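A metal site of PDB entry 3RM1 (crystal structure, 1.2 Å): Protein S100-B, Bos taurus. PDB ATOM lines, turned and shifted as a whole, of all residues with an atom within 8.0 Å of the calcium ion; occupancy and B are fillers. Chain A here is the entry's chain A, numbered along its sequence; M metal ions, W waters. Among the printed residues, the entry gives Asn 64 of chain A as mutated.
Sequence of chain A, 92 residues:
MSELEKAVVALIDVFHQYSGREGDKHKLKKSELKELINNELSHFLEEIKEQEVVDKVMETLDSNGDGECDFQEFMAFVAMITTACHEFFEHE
The side-chain carboxylate (OD2) of Asp 62 lies within hydrogen-bond range of the backbone NH (N) of Gly 67 (2.8 Å).
The side-chain carboxylate (OD2) of Asp 66 lies within salt-bridge range of the side-chain amino group (NZ) of Lys 27 (2.8 Å).
The backbone NH (N) of Glu 73 sits at hydrogen-bond distance from the side-chain carboxylate (OD1) of Asp 70.
N of Gly 65 sits close to OD1 of Asp 62, at 3.2 Å.
The side-chain carboxylate (OE2) of Glu 73 sits close to the backbone NH (N) of Ser 63, 3.2 Å away.
The nearest printed residue that does not touch the calcium ion is Asp 70 (4.4 Å).
The calcium ion is bound by the side-chain carboxylate (OD1) of Asp 62 (2.3 Å), the backbone carbonyl oxygen (O) of Glu 68 (2.3 Å), water W1 (2.3 Å), the side-chain amide oxygen (OD1) of Asn 64 (2.3 Å), the side-chain carboxylate (OD1) of Asp 66 (2.4 Å), the side-chain carboxylate (OE1) of Glu 73 (2.4 Å) and the side-chain carboxylate (OE2) of Glu 73 (2.6 Å).
The calcium ion has seven donor atoms within binding distance.
Water W1 bridges the side-chain carboxylate (OD2) of Asp 66 (2.7 Å) and the side-chain carboxylate (OD2) of Asp 70 (2.7 Å).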
ATOM      1  N   LYS A  27      14.105  24.524   1.660  1.00  0.00           N
ATOM      2  CA  LYS A  27      14.820  24.171   2.878  1.00  0.00           C
ATOM      3  C   LYS A  27      14.171  24.752   4.094  1.00  0.00           C
ATOM      4  O   LYS A  27      13.529  25.829   4.005  1.00  0.00           O
ATOM      5  CB  LYS A  27      16.301  24.596   2.823  1.00  0.00           C
ATOM      6  CG  LYS A  27      17.053  24.041   1.628  1.00  0.00           C
ATOM      7  CD  LYS A  27      18.503  24.540   1.651  1.00  0.00           C
ATOM      8  CE  LYS A  27      19.289  24.216   0.363  1.00  0.00           C
ATOM      9  NZ  LYS A  27      20.608  24.950   0.374  1.00  0.00           N
ATOM     10  N   LEU A  28      14.349  24.038   5.199  1.00  0.00           N
ATOM     11  CA  LEU A  28      13.934  24.478   6.530  1.00  0.00           C
ATOM     12  C   LEU A  28      15.038  25.246   7.225  1.00  0.00           C
ATOM     13  O   LEU A  28      16.101  24.701   7.504  1.00  0.00           O
ATOM     14  CB  LEU A  28      13.611  23.291   7.413  1.00  0.00           C
ATOM     15  CG  LEU A  28      12.517  22.343   6.939  1.00  0.00           C
ATOM     16  CD1 LEU A  28      12.548  21.005   7.685  1.00  0.00           C
ATOM     17  CD2 LEU A  28      11.096  22.944   7.054  1.00  0.00           C
ATOM     18  N   MET A  58      19.270  21.379  14.619  1.00  0.00           N
ATOM     19  CA  MET A  58      19.740  21.757  13.268  1.00  0.00           C
ATOM     20  C   MET A  58      21.142  21.258  12.993  1.00  0.00           C
ATOM     21  O   MET A  58      21.424  20.729  11.930  1.00  0.00           O
ATOM     22  CB  MET A  58      19.678  23.266  13.030  1.00  0.00           C
ATOM     23  CG  MET A  58      20.178  23.675  11.661  1.00  0.00           C
ATOM     24  SD  MET A  58      19.105  23.079  10.271  1.00  0.00           S
ATOM     25  CE  MET A  58      17.795  24.287  10.303  1.00  0.00           C
ATOM     26  N   LEU A  61      20.970  17.561  12.148  1.00  0.00           N
ATOM     27  CA  LEU A  61      20.330  17.232  10.869  1.00  0.00           C
ATOM     28  C   LEU A  61      21.020  17.811   9.640  1.00  0.00           C
ATOM     29  O   LEU A  61      20.859  17.272   8.562  1.00  0.00           O
ATOM     30  CB  LEU A  61      18.864  17.664  10.882  1.00  0.00           C
ATOM     31  CG  LEU A  61      17.984  17.077  11.991  1.00  0.00           C
ATOM     32  CD1 LEU A  61      16.553  17.551  11.796  1.00  0.00           C
ATOM     33  CD2 LEU A  61      18.099  15.543  12.017  1.00  0.00           C
ATOM     34  N   ASP A  62      21.774  18.889   9.805  1.00  0.00           N
ATOM     35  CA  ASP A  62      22.367  19.616   8.675  1.00  0.00           C
ATOM     36  C   ASP A  62      23.658  18.939   8.240  1.00  0.00           C
ATOM     37  O   ASP A  62      24.772  19.466   8.434  1.00  0.00           O
ATOM     38  CB  ASP A  62      22.584  21.074   9.069  1.00  0.00           C
ATOM     39  CG  ASP A  62      23.266  21.866   7.993  1.00  0.00           C
ATOM     40  OD1 ASP A  62      23.085  21.552   6.800  1.00  0.00           O
ATOM     41  OD2 ASP A  62      23.959  22.828   8.337  1.00  0.00           O
ATOM     42  N   SER A  63      23.515  17.802   7.584  1.00  0.00           N
ATOM     43  CA  SER A  63      24.671  16.996   7.176  1.00  0.00           C
ATOM     44  C   SER A  63      25.578  17.716   6.196  1.00  0.00           C
ATOM     45  O   SER A  63      26.795  17.478   6.225  1.00  0.00           O
ATOM     46  CB  SER A  63      24.213  15.683   6.579  1.00  0.00           C
ATOM     47  OG  SER A  63      23.594  14.877   7.564  1.00  0.00           O
ATOM     48  N   ASN A  64      25.042  18.568   5.313  1.00  0.00           N
ATOM     49  CA  ASN A  64      25.898  19.254   4.340  1.00  0.00           C
ATOM     50  C   ASN A  64      26.456  20.599   4.801  1.00  0.00           C
ATOM     51  O   ASN A  64      27.209  21.232   4.068  1.00  0.00           O
ATOM     52  CB  ASN A  64      25.231  19.405   2.962  1.00  0.00           C
ATOM     53  CG  ASN A  64      24.283  20.595   2.885  1.00  0.00           C
ATOM     54  OD1 ASN A  64      23.760  21.048   3.874  1.00  0.00           O
ATOM     55  ND2 ASN A  64      24.067  21.103   1.679  1.00  0.00           N
ATOM     56  N   GLY A  65      26.092  21.046   6.007  1.00  0.00           N
ATOM     57  CA  GLY A  65      26.677  22.226   6.638  1.00  0.00           C
ATOM     58  C   GLY A  65      26.224  23.584   6.133  1.00  0.00           C
ATOM     59  O   GLY A  65      26.855  24.596   6.417  1.00  0.00           O
ATOM     60  N   ASP A  66      25.141  23.637   5.377  1.00  0.00           N
ATOM     61  CA  ASP A  66      24.671  24.903   4.833  1.00  0.00           C
ATOM     62  C   ASP A  66      23.716  25.684   5.754  1.00  0.00           C
ATOM     63  O   ASP A  66      23.210  26.739   5.371  1.00  0.00           O
ATOM     64  CB  ASP A  66      24.078  24.747   3.419  1.00  0.00           C
ATOM     65  CG  ASP A  66      22.777  23.980   3.400  1.00  0.00           C
ATOM     66  OD1 ASP A  66      22.215  23.612   4.475  1.00  0.00           O
ATOM     67  OD2 ASP A  66      22.311  23.696   2.262  1.00  0.00           O
ATOM     68  N   GLY A  67      23.521  25.181   6.974  1.00  0.00           N
ATOM     69  CA  GLY A  67      22.710  25.926   7.958  1.00  0.00           C
ATOM     70  C   GLY A  67      21.205  25.706   7.852  1.00  0.00           C
ATOM     71  O   GLY A  67      20.440  26.240   8.649  1.00  0.00           O
ATOM     72  N   GLU A  68      20.769  24.907   6.875  1.00  0.00           N
ATOM     73  CA  GLU A  68      19.347  24.604   6.718  1.00  0.00           C
ATOM     74  C   GLU A  68      19.158  23.123   6.551  1.00  0.00           C
ATOM     75  O   GLU A  68      20.116  22.404   6.248  1.00  0.00           O
ATOM     76  CB  GLU A  68      18.723  25.364   5.538  1.00  0.00           C
ATOM     77  CG  GLU A  68      18.873  26.897   5.679  1.00  0.00           C
ATOM     78  CD  GLU A  68      17.789  27.700   4.995  1.00  0.00           C
ATOM     79  OE1 GLU A  68      16.686  27.195   4.800  1.00  0.00           O
ATOM     80  OE2 GLU A  68      18.039  28.878   4.705  1.00  0.00           O
ATOM     81  N   CYS A  69      17.917  22.659   6.742  1.00  0.00           N
ATOM     82  CA  CYS A  69      17.608  21.248   6.550  1.00  0.00           C
ATOM     83  C   CYS A  69      16.871  21.082   5.219  1.00  0.00           C
ATOM     84  O   CYS A  69      15.725  21.549   5.073  1.00  0.00           O
ATOM     85  CB  CYS A  69      16.727  20.771   7.709  1.00  0.00           C
ATOM     86  SG  CYS A  69      16.303  19.010   7.651  1.00  0.00           S
ATOM     87  N   ASP A  70      17.496  20.404   4.248  1.00  0.00           N
ATOM     88  CA  ASP A  70      16.859  20.173   2.955  1.00  0.00           C
ATOM     89  C   ASP A  70      16.031  18.890   2.989  1.00  0.00           C
ATOM     90  O   ASP A  70      15.870  18.270   4.063  1.00  0.00           O
ATOM     91  CB  ASP A  70      17.893  20.203   1.815  1.00  0.00           C
ATOM     92  CG  ASP A  70      18.927  19.102   1.925  1.00  0.00           C
ATOM     93  OD1 ASP A  70      18.664  18.013   2.494  1.00  0.00           O
ATOM     94  OD2 ASP A  70      20.021  19.348   1.405  1.00  0.00           O
ATOM     95  N   PHE A  71      15.452  18.534   1.853  1.00  0.00           N
ATOM     96  CA  PHE A  71      14.531  17.426   1.875  1.00  0.00           C
ATOM     97  C   PHE A  71      15.219  16.092   2.174  1.00  0.00           C
ATOM     98  O   PHE A  71      14.657  15.263   2.880  1.00  0.00           O
ATOM     99  CB  PHE A  71      13.748  17.328   0.573  1.00  0.00           C
ATOM    100  CG  PHE A  71      12.683  16.288   0.640  1.00  0.00           C
ATOM    101  CD1 PHE A  71      11.553  16.508   1.444  1.00  0.00           C
ATOM    102  CD2 PHE A  71      12.806  15.071  -0.039  1.00  0.00           C
ATOM    103  CE1 PHE A  71      10.547  15.570   1.565  1.00  0.00           C
ATOM    104  CE2 PHE A  71      11.797  14.098   0.063  1.00  0.00           C
ATOM    105  CZ  PHE A  71      10.638  14.369   0.861  1.00  0.00           C
ATOM    106  N   GLU A  73      17.886  15.719   4.072  1.00  0.00           N
ATOM    107  CA  GLU A  73      18.222  15.744   5.474  1.00  0.00           C
ATOM    108  C   GLU A  73      16.947  15.562   6.326  1.00  0.00           C
ATOM    109  O   GLU A  73      16.993  14.915   7.373  1.00  0.00           O
ATOM    110  CB  GLU A  73      18.900  17.084   5.799  1.00  0.00           C
ATOM    111  CG  GLU A  73      20.310  17.170   5.184  1.00  0.00           C
ATOM    112  CD  GLU A  73      20.830  18.586   5.126  1.00  0.00           C
ATOM    113  OE1 GLU A  73      20.048  19.574   5.224  1.00  0.00           O
ATOM    114  OE2 GLU A  73      22.060  18.776   4.956  1.00  0.00           O
ATOM    115  N   PHE A  74      15.806  16.073   5.849  1.00  0.00           N
ATOM    116  CA  PHE A  74      14.531  15.822   6.492  1.00  0.00           C
ATOM    117  C   PHE A  74      14.150  14.341   6.438  1.00  0.00           C
ATOM    118  O   PHE A  74      13.684  13.774   7.443  1.00  0.00           O
ATOM    119  CB  PHE A  74      13.444  16.677   5.859  1.00  0.00           C
ATOM    120  CG  PHE A  74      12.070  16.408   6.405  1.00  0.00           C
ATOM    121  CD1 PHE A  74      11.740  16.791   7.700  1.00  0.00           C
ATOM    122  CD2 PHE A  74      11.126  15.756   5.640  1.00  0.00           C
ATOM    123  CE1 PHE A  74      10.485  16.540   8.215  1.00  0.00           C
ATOM    124  CE2 PHE A  74       9.871  15.500   6.164  1.00  0.00           C
ATOM    125  CZ  PHE A  74       9.563  15.913   7.462  1.00  0.00           C
HETATM  126 CA    CA M   1      21.712  21.315   4.972  1.00  0.00          CA
HETATM  127  O   HOH W   1      20.758  21.565   2.853  1.00  0.00           O
